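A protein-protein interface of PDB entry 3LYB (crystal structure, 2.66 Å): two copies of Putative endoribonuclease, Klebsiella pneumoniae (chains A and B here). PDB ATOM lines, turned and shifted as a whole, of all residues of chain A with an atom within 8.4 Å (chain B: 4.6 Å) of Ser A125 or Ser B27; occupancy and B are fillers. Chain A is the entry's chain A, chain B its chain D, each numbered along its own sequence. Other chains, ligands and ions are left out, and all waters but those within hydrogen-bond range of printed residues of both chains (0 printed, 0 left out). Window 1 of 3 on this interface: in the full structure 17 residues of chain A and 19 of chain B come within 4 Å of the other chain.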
ATOM      1  N   ILE A  95      38.548   8.895  -5.550  1.00  0.00           N
ATOM      2  CA  ILE A  95      37.748   8.008  -4.725  1.00  0.00           C
ATOM      3  C   ILE A  95      36.221   8.139  -4.900  1.00  0.00           C
ATOM      4  O   ILE A  95      35.494   7.140  -4.745  1.00  0.00           O
ATOM      5  CB  ILE A  95      38.124   8.150  -3.235  1.00  0.00           C
ATOM      6  CG1 ILE A  95      38.589   9.567  -2.917  1.00  0.00           C
ATOM      7  CG2 ILE A  95      39.258   7.190  -2.894  1.00  0.00           C
ATOM      8  CD1 ILE A  95      37.568  10.388  -2.228  1.00  0.00           C
ATOM      9  N   LYS A  96      35.762   9.352  -5.248  1.00  0.00           N
ATOM     10  CA  LYS A  96      34.338   9.706  -5.264  1.00  0.00           C
ATOM     11  C   LYS A  96      33.904  10.472  -6.518  1.00  0.00           C
ATOM     12  O   LYS A  96      34.553  11.447  -6.956  1.00  0.00           O
ATOM     13  CB  LYS A  96      34.026  10.559  -4.042  1.00  0.00           C
ATOM     14  CG  LYS A  96      32.639  11.149  -4.015  1.00  0.00           C
ATOM     15  CD  LYS A  96      32.537  12.268  -2.996  1.00  0.00           C
ATOM     16  CE  LYS A  96      31.089  12.634  -2.699  1.00  0.00           C
ATOM     17  NZ  LYS A  96      30.513  11.679  -1.727  1.00  0.00           N
ATOM     18  N   LEU A  97      32.787  10.042  -7.088  1.00  0.00           N
ATOM     19  CA  LEU A  97      32.248  10.742  -8.232  1.00  0.00           C
ATOM     20  C   LEU A  97      30.794  11.091  -7.981  1.00  0.00           C
ATOM     21  O   LEU A  97      30.021  10.265  -7.460  1.00  0.00           O
ATOM     22  CB  LEU A  97      32.379   9.898  -9.496  1.00  0.00           C
ATOM     23  CG  LEU A  97      33.755   9.533 -10.056  1.00  0.00           C
ATOM     24  CD1 LEU A  97      33.566   8.767 -11.364  1.00  0.00           C
ATOM     25  CD2 LEU A  97      34.654  10.696 -10.310  1.00  0.00           C
ATOM     26  N   VAL A  98      30.431  12.329  -8.307  1.00  0.00           N
ATOM     27  CA  VAL A  98      29.018  12.696  -8.358  1.00  0.00           C
ATOM     28  C   VAL A  98      28.726  12.985  -9.823  1.00  0.00           C
ATOM     29  O   VAL A  98      29.487  13.705 -10.497  1.00  0.00           O
ATOM     30  CB  VAL A  98      28.599  13.858  -7.362  1.00  0.00           C
ATOM     31  CG1 VAL A  98      27.063  14.106  -7.398  1.00  0.00           C
ATOM     32  CG2 VAL A  98      29.029  13.549  -5.933  1.00  0.00           C
ATOM     33  N   GLN A  99      27.677  12.346 -10.328  1.00  0.00           N
ATOM     34  CA  GLN A  99      27.422  12.263 -11.769  1.00  0.00           C
ATOM     35  C   GLN A  99      25.989  12.682 -12.075  1.00  0.00           C
ATOM     36  O   GLN A  99      25.014  12.034 -11.607  1.00  0.00           O
ATOM     37  CB  GLN A  99      27.666  10.831 -12.259  1.00  0.00           C
ATOM     38  CG  GLN A  99      29.159  10.391 -12.265  1.00  0.00           C
ATOM     39  CD  GLN A  99      29.359   9.033 -11.631  1.00  0.00           C
ATOM     40  OE1 GLN A  99      30.117   8.192 -12.145  1.00  0.00           O
ATOM     41  NE2 GLN A  99      28.641   8.788 -10.520  1.00  0.00           N
ATOM     42  N   PHE A 101      23.073  13.737 -14.882  1.00  0.00           N
ATOM     43  CA  PHE A 101      22.593  13.403 -16.215  1.00  0.00           C
ATOM     44  C   PHE A 101      21.350  14.199 -16.512  1.00  0.00           C
ATOM     45  O   PHE A 101      20.592  14.526 -15.578  1.00  0.00           O
ATOM     46  CB  PHE A 101      22.186  11.952 -16.230  1.00  0.00           C
ATOM     47  CG  PHE A 101      23.334  11.008 -16.166  1.00  0.00           C
ATOM     48  CD1 PHE A 101      23.961  10.742 -14.957  1.00  0.00           C
ATOM     49  CD2 PHE A 101      23.768  10.357 -17.316  1.00  0.00           C
ATOM     50  CE1 PHE A 101      25.046   9.857 -14.916  1.00  0.00           C
ATOM     51  CE2 PHE A 101      24.810   9.481 -17.278  1.00  0.00           C
ATOM     52  CZ  PHE A 101      25.460   9.218 -16.088  1.00  0.00           C
ATOM     53  N   PHE A 107      22.725   6.398 -18.857  1.00  0.00           N
ATOM     54  CA  PHE A 107      23.591   5.729 -17.888  1.00  0.00           C
ATOM     55  C   PHE A 107      24.393   4.519 -18.449  1.00  0.00           C
ATOM     56  O   PHE A 107      25.610   4.485 -18.292  1.00  0.00           O
ATOM     57  CB  PHE A 107      22.857   5.341 -16.597  1.00  0.00           C
ATOM     58  CG  PHE A 107      23.755   4.677 -15.603  1.00  0.00           C
ATOM     59  CD1 PHE A 107      24.644   5.440 -14.836  1.00  0.00           C
ATOM     60  CD2 PHE A 107      23.773   3.283 -15.483  1.00  0.00           C
ATOM     61  CE1 PHE A 107      25.505   4.841 -13.943  1.00  0.00           C
ATOM     62  CE2 PHE A 107      24.648   2.654 -14.583  1.00  0.00           C
ATOM     63  CZ  PHE A 107      25.524   3.430 -13.813  1.00  0.00           C
ATOM     64  N   TYR A 110      27.293   5.861 -20.345  1.00  0.00           N
ATOM     65  CA  TYR A 110      28.259   6.453 -19.469  1.00  0.00           C
ATOM     66  C   TYR A 110      29.026   5.370 -18.691  1.00  0.00           C
ATOM     67  O   TYR A 110      30.233   5.472 -18.491  1.00  0.00           O
ATOM     68  CB  TYR A 110      27.601   7.449 -18.513  1.00  0.00           C
ATOM     69  CG  TYR A 110      28.531   7.841 -17.394  1.00  0.00           C
ATOM     70  CD1 TYR A 110      29.608   8.666 -17.632  1.00  0.00           C
ATOM     71  CD2 TYR A 110      28.380   7.311 -16.132  1.00  0.00           C
ATOM     72  CE1 TYR A 110      30.507   8.996 -16.608  1.00  0.00           C
ATOM     73  CE2 TYR A 110      29.241   7.627 -15.125  1.00  0.00           C
ATOM     74  CZ  TYR A 110      30.314   8.465 -15.363  1.00  0.00           C
ATOM     75  OH  TYR A 110      31.178   8.791 -14.344  1.00  0.00           O
ATOM     76  N   ARG A 114      32.981   4.707 -18.041  1.00  0.00           N
ATOM     77  CA  ARG A 114      33.570   4.799 -16.704  1.00  0.00           C
ATOM     78  C   ARG A 114      34.389   3.549 -16.360  1.00  0.00           C
ATOM     79  O   ARG A 114      35.416   3.664 -15.689  1.00  0.00           O
ATOM     80  CB  ARG A 114      32.518   5.111 -15.625  1.00  0.00           C
ATOM     81  CG  ARG A 114      33.112   5.426 -14.266  1.00  0.00           C
ATOM     82  CD  ARG A 114      32.071   5.646 -13.192  1.00  0.00           C
ATOM     83  NE  ARG A 114      31.213   4.470 -13.020  1.00  0.00           N
ATOM     84  CZ  ARG A 114      30.109   4.426 -12.269  1.00  0.00           C
ATOM     85  NH1 ARG A 114      29.679   5.504 -11.598  1.00  0.00           N
ATOM     86  NH2 ARG A 114      29.419   3.293 -12.212  1.00  0.00           N
ATOM     87  N   PRO A 122      37.473   0.909  -8.425  1.00  0.00           N
ATOM     88  CA  PRO A 122      36.277   1.777  -8.614  1.00  0.00           C
ATOM     89  C   PRO A 122      35.961   2.760  -7.460  1.00  0.00           C
ATOM     90  O   PRO A 122      36.140   2.412  -6.280  1.00  0.00           O
ATOM     91  CB  PRO A 122      35.116   0.775  -8.799  1.00  0.00           C
ATOM     92  CG  PRO A 122      35.728  -0.641  -8.661  1.00  0.00           C
ATOM     93  CD  PRO A 122      37.215  -0.466  -8.901  1.00  0.00           C
ATOM     94  N   PRO A 123      35.481   3.984  -7.811  1.00  0.00           N
ATOM     95  CA  PRO A 123      35.187   5.013  -6.814  1.00  0.00           C
ATOM     96  C   PRO A 123      33.804   4.816  -6.202  1.00  0.00           C
ATOM     97  O   PRO A 123      33.009   3.995  -6.682  1.00  0.00           O
ATOM     98  CB  PRO A 123      35.198   6.289  -7.644  1.00  0.00           C
ATOM     99  CG  PRO A 123      34.647   5.856  -8.974  1.00  0.00           C
ATOM    100  CD  PRO A 123      35.015   4.397  -9.158  1.00  0.00           C
ATOM    101  N   VAL A 124      33.536   5.551  -5.136  1.00  0.00           N
ATOM    102  CA  VAL A 124      32.215   5.656  -4.572  1.00  0.00           C
ATOM    103  C   VAL A 124      31.376   6.531  -5.520  1.00  0.00           C
ATOM    104  O   VAL A 124      31.899   7.441  -6.153  1.00  0.00           O
ATOM    105  CB  VAL A 124      32.345   6.212  -3.137  1.00  0.00           C
ATOM    106  CG1 VAL A 124      31.209   7.111  -2.759  1.00  0.00           C
ATOM    107  CG2 VAL A 124      32.489   5.060  -2.135  1.00  0.00           C
ATOM    108  N   SER A 125      30.084   6.236  -5.642  1.00  0.00           N
ATOM    109  CA  SER A 125      29.277   6.796  -6.728  1.00  0.00           C
ATOM    110  C   SER A 125      27.887   7.333  -6.327  1.00  0.00           C
ATOM    111  O   SER A 125      27.159   6.698  -5.577  1.00  0.00           O
ATOM    112  CB  SER A 125      29.123   5.724  -7.806  1.00  0.00           C
ATOM    113  OG  SER A 125      28.286   6.144  -8.872  1.00  0.00           O
ATOM    114  N   THR A 126      27.532   8.507  -6.838  1.00  0.00           N
ATOM    115  CA  THR A 126      26.159   9.017  -6.753  1.00  0.00           C
ATOM    116  C   THR A 126      25.759   9.442  -8.151  1.00  0.00           C
ATOM    117  O   THR A 126      26.544  10.045  -8.855  1.00  0.00           O
ATOM    118  CB  THR A 126      26.027  10.240  -5.808  1.00  0.00           C
ATOM    119  OG1 THR A 126      26.538   9.917  -4.522  1.00  0.00           O
ATOM    120  CG2 THR A 126      24.576  10.617  -5.612  1.00  0.00           C
ATOM    121  N   VAL A 127      24.538   9.132  -8.537  1.00  0.00           N
ATOM    122  CA  VAL A 127      24.043   9.354  -9.877  1.00  0.00           C
ATOM    123  C   VAL A 127      22.617   9.897  -9.806  1.00  0.00           C
ATOM    124  O   VAL A 127      21.718   9.260  -9.233  1.00  0.00           O
ATOM    125  CB  VAL A 127      23.979   8.022 -10.632  1.00  0.00           C
ATOM    126  CG1 VAL A 127      23.176   8.164 -11.920  1.00  0.00           C
ATOM    127  CG2 VAL A 127      25.395   7.461 -10.891  1.00  0.00           C
ATOM    128  N   VAL A 128      22.402  11.061 -10.403  1.00  0.00           N
ATOM    129  CA  VAL A 128      21.073  11.653 -10.462  1.00  0.00           C
ATOM    130  C   VAL A 128      20.779  12.247 -11.814  1.00  0.00           C
ATOM    131  O   VAL A 128      21.691  12.636 -12.546  1.00  0.00           O
ATOM    132  CB  VAL A 128      20.876  12.781  -9.436  1.00  0.00           C
ATOM    133  CG1 VAL A 128      20.848  12.218  -8.022  1.00  0.00           C
ATOM    134  CG2 VAL A 128      21.951  13.823  -9.572  1.00  0.00           C
ATOM    135  N   GLU A 144      31.498  15.460 -11.015  1.00  0.00           N
ATOM    136  CA  GLU A 144      32.293  16.101  -9.959  1.00  0.00           C
ATOM    137  C   GLU A 144      33.169  15.039  -9.321  1.00  0.00           C
ATOM    138  O   GLU A 144      32.663  14.054  -8.792  1.00  0.00           O
ATOM    139  CB  GLU A 144      31.403  16.745  -8.881  1.00  0.00           C
ATOM    140  CG  GLU A 144      32.132  17.350  -7.649  1.00  0.00           C
ATOM    141  CD  GLU A 144      31.208  17.521  -6.421  1.00  0.00           C
ATOM    142  OE1 GLU A 144      30.195  18.266  -6.513  1.00  0.00           O
ATOM    143  OE2 GLU A 144      31.477  16.909  -5.347  1.00  0.00           O
ATOM    144  N   TYR B  14      31.092  -0.183  -9.063  1.00  0.00           N
ATOM    145  CA  TYR B  14      31.454   0.809  -7.995  1.00  0.00           C
ATOM    146  C   TYR B  14      31.455   0.240  -6.578  1.00  0.00           C
ATOM    147  O   TYR B  14      30.887  -0.828  -6.341  1.00  0.00           O
ATOM    148  CB  TYR B  14      30.546   2.046  -8.055  1.00  0.00           C
ATOM    149  CG  TYR B  14      29.123   1.803  -7.621  1.00  0.00           C
ATOM    150  CD1 TYR B  14      28.169   1.385  -8.531  1.00  0.00           C
ATOM    151  CD2 TYR B  14      28.727   2.003  -6.289  1.00  0.00           C
ATOM    152  CE1 TYR B  14      26.871   1.173  -8.133  1.00  0.00           C
ATOM    153  CE2 TYR B  14      27.428   1.788  -5.883  1.00  0.00           C
ATOM    154  CZ  TYR B  14      26.511   1.378  -6.815  1.00  0.00           C
ATOM    155  OH  TYR B  14      25.219   1.165  -6.450  1.00  0.00           O
ATOM    156  N   ALA B  15      32.060   1.003  -5.653  1.00  0.00           N
ATOM    157  CA  ALA B  15      32.306   0.596  -4.255  1.00  0.00           C
ATOM    158  C   ALA B  15      31.273   1.103  -3.235  1.00  0.00           C
ATOM    159  O   ALA B  15      31.152   2.318  -3.010  1.00  0.00           O
ATOM    160  CB  ALA B  15      33.699   1.025  -3.825  1.00  0.00           C
ATOM    161  N   ALA B  16      30.564   0.169  -2.589  1.00  0.00           N
ATOM    162  CA  ALA B  16      29.588   0.502  -1.541  1.00  0.00           C
ATOM    163  C   ALA B  16      30.064   1.651  -0.622  1.00  0.00           C
ATOM    164  O   ALA B  16      29.327   2.617  -0.399  1.00  0.00           O
ATOM    165  CB  ALA B  16      29.219  -0.746  -0.743  1.00  0.00           C
ATOM    166  N   PHE B  25      33.457   7.694   2.720  1.00  0.00           N
ATOM    167  CA  PHE B  25      32.452   8.051   1.716  1.00  0.00           C
ATOM    168  C   PHE B  25      31.612   6.854   1.336  1.00  0.00           C
ATOM    169  O   PHE B  25      32.120   5.802   0.987  1.00  0.00           O
ATOM    170  CB  PHE B  25      33.121   8.603   0.460  1.00  0.00           C
ATOM    171  CG  PHE B  25      33.859   9.867   0.691  1.00  0.00           C
ATOM    172  CD1 PHE B  25      35.255   9.854   0.823  1.00  0.00           C
ATOM    173  CD2 PHE B  25      33.168  11.074   0.813  1.00  0.00           C
ATOM    174  CE1 PHE B  25      35.978  11.046   1.060  1.00  0.00           C
ATOM    175  CE2 PHE B  25      33.863  12.284   1.044  1.00  0.00           C
ATOM    176  CZ  PHE B  25      35.280  12.273   1.169  1.00  0.00           C
ATOM    177  N   LEU B  26      30.306   7.023   1.431  1.00  0.00           N
ATOM    178  CA  LEU B  26      29.376   6.036   0.925  1.00  0.00           C
ATOM    179  C   LEU B  26      28.860   6.494  -0.406  1.00  0.00           C
ATOM    180  O   LEU B  26      28.714   7.703  -0.655  1.00  0.00           O
ATOM    181  CB  LEU B  26      28.197   5.865   1.870  1.00  0.00           C
ATOM    182  CG  LEU B  26      28.425   4.980   3.088  1.00  0.00           C
ATOM    183  CD1 LEU B  26      29.321   5.666   4.125  1.00  0.00           C
ATOM    184  CD2 LEU B  26      27.083   4.593   3.695  1.00  0.00           C
ATOM    185  N   SER B  27      28.603   5.518  -1.265  1.00  0.00           N
ATOM    186  CA  SER B  27      27.806   5.743  -2.444  1.00  0.00           C
ATOM    187  C   SER B  27      26.403   6.165  -2.039  1.00  0.00           C
ATOM    188  O   SER B  27      25.945   5.820  -0.943  1.00  0.00           O
ATOM    189  CB  SER B  27      27.739   4.474  -3.277  1.00  0.00           C
ATOM    190  OG  SER B  27      28.997   4.226  -3.879  1.00  0.00           O
ATOM    191  N   GLY B  28      25.744   6.922  -2.927  1.00  0.00           N
ATOM    192  CA  GLY B  28      24.307   7.171  -2.861  1.00  0.00           C
ATOM    193  C   GLY B  28      23.599   5.828  -2.772  1.00  0.00           C
ATOM    194  O   GLY B  28      24.007   4.857  -3.398  1.00  0.00           O
ATOM    195  N   ILE B  29      22.586   5.761  -1.924  1.00  0.00           N
ATOM    196  CA  ILE B  29      21.913   4.513  -1.633  1.00  0.00           C
ATOM    197  C   ILE B  29      20.426   4.648  -1.968  1.00  0.00           C
ATOM    198  O   ILE B  29      19.789   5.669  -1.648  1.00  0.00           O
ATOM    199  CB  ILE B  29      22.189   4.066  -0.168  1.00  0.00           C
ATOM    200  CG1 ILE B  29      23.565   3.412  -0.087  1.00  0.00           C
ATOM    201  CG2 ILE B  29      21.140   3.074   0.330  1.00  0.00           C
ATOM    202  CD1 ILE B  29      24.014   3.053   1.336  1.00  0.00           C
ATOM    203  N   VAL B 143      19.813   8.751  -0.663  1.00  0.00           N
ATOM    204  CA  VAL B 143      20.673   9.459   0.310  1.00  0.00           C
ATOM    205  C   VAL B 143      22.153   9.115   0.170  1.00  0.00           C
ATOM    206  O   VAL B 143      22.532   7.941   0.088  1.00  0.00           O
ATOM    207  CB  VAL B 143      20.231   9.239   1.758  1.00  0.00           C
ATOM    208  CG1 VAL B 143      21.120  10.025   2.706  1.00  0.00           C
ATOM    209  CG2 VAL B 143      18.811   9.671   1.924  1.00  0.00           C
ATOM    210  N   GLU B 144      22.985  10.145   0.107  1.00  0.00           N
ATOM    211  CA  GLU B 144      24.424   9.945   0.042  1.00  0.00           C
ATOM    212  C   GLU B 144      24.969  10.340   1.393  1.00  0.00           C
ATOM    213  O   GLU B 144      24.655  11.426   1.885  1.00  0.00           O
ATOM    214  CB  GLU B 144      25.045  10.806  -1.054  1.00  0.00           C
ATOM    215  CG  GLU B 144      26.540  10.714  -1.146  1.00  0.00           C
ATOM    216  CD  GLU B 144      27.129  11.988  -1.670  1.00  0.00           C
ATOM    217  OE1 GLU B 144      27.197  12.127  -2.907  1.00  0.00           O
ATOM    218  OE2 GLU B 144      27.497  12.874  -0.860  1.00  0.00           O
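Of the 10 printed residues of chain B, 7 touch a printed residue of chain A. Printed residues of chain B that touch a printed residue of chain A: Tyr B14, Ala B15, Phe B25, Leu B26, Ser B27, Gly B28 and Glu B144. Hydrophobic or aromatic side chains of chain B within 4 Å of the printed part of chain A: Tyr B14, Ala B15 and Phe B25. Among the printed residues, Asp or Glu carboxylates within 4 Å of a Lys or Arg side-chain nitrogen of the other chain: Lys A96 with Glu B144 (3.4 Å).
The side-chain hydroxyl (OG) of Ser B27 lies within hydrogen-bond range of the backbone carbonyl oxygen (O) of Ala B15. The backbone NH (N) of Gln A99 lies within hydrogen-bond range of the backbone carbonyl oxygen (O) of Thr A126. The backbone carbonyl oxygen (O) of Leu A97 is in hydrogen-bond range of the backbone NH (N) of Thr A126, at 3.1 Å. The backbone carbonyl oxygen of Ile A95 sits at hydrogen-bond distance from the backbone NH of Val A124 (2.6 Å). NH1 of Arg A114 sits at hydrogen-bond distance from OG of Ser A125 (3.1 Å). N of Ser B27 sits at hydrogen-bond distance from O of Ala B16 (3.1 Å).
The side-chain carboxylate of Glu B144 lies within salt-bridge range of the side-chain amino group of Lys A96 (3.4 Å). N of Ser A125 is in hydrogen-bond range of OG of Ser B27. OE1 of Glu B144 sits at hydrogen-bond distance from OG1 of Thr A126 (2.8 Å). The side-chain hydroxyl (OG1) of Thr A126 is in hydrogen-bond range of the backbone NH (N) of Gly B28, at 3.5 Å. N of Ala B15 sits at hydrogen-bond distance from O of Pro A123 (3.3 Å). The backbone carbonyl oxygen of Ser A125 sits at hydrogen-bond distance from the backbone NH of Gly B28 (3.0 Å).
CD2 of Phe B25 touches NZ of Lys A96, 3.7 Å away. Val A98 touches Glu B144 (CG2 to OE1, 3.8 Å). Tyr B14 touches Pro A122 (CA to CB, 3.7 Å). Ala B15 touches Pro A122. Pro A123 touches Tyr B14. Val A124 touches Ala B15. Phe B25 touches Val A124 (O to CG2, 3.2 Å). O of Leu B26 touches CG1 of Val A124, at 3.3 Å. CG1 of Val A124 touches N of Ser B27, at 3.4 Å. CG of Tyr B14 touches CB of Ser A125, at 3.9 Å.
Position printed for both chains: 144. Of the 17 pairs that touch across the chains among the printed residues, none has its exchanged pair printed and touching as well.
Printed residues of chain B within 4 Å of Pro A122: Tyr B14 and Ala B15. Of chain B, only Tyr B14 (3.9 Å), Ser B27 (2.9 Å) and Gly B28 (3.0 Å) come within 4 Å of Ser A125. Of the printed residues of chain A, Ala B15 touches Pro A122 (3.7 Å), Pro A123 (3.3 Å) and Val A124 (3.2 Å). Ala B16 touches none of the printed residues of chain A. Of the printed residues of chain A, Phe B25 touches Ile A95, Lys A96 and Val A124. Ser B27 touches just these residues of chain A: Val A124 (3.4 Å) and Ser A125 (2.9 Å). Of the printed residues of chain A, Gly B28 touches Ser A125 (3.0 Å) and Thr A126 (3.5 Å). The nearest printed residue of chain B that does not touch Ser A125 is Ala B15 (4.8 Å). The nearest residue of chain A that does not touch Ser B27 is Thr A126 (4.5 Å).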
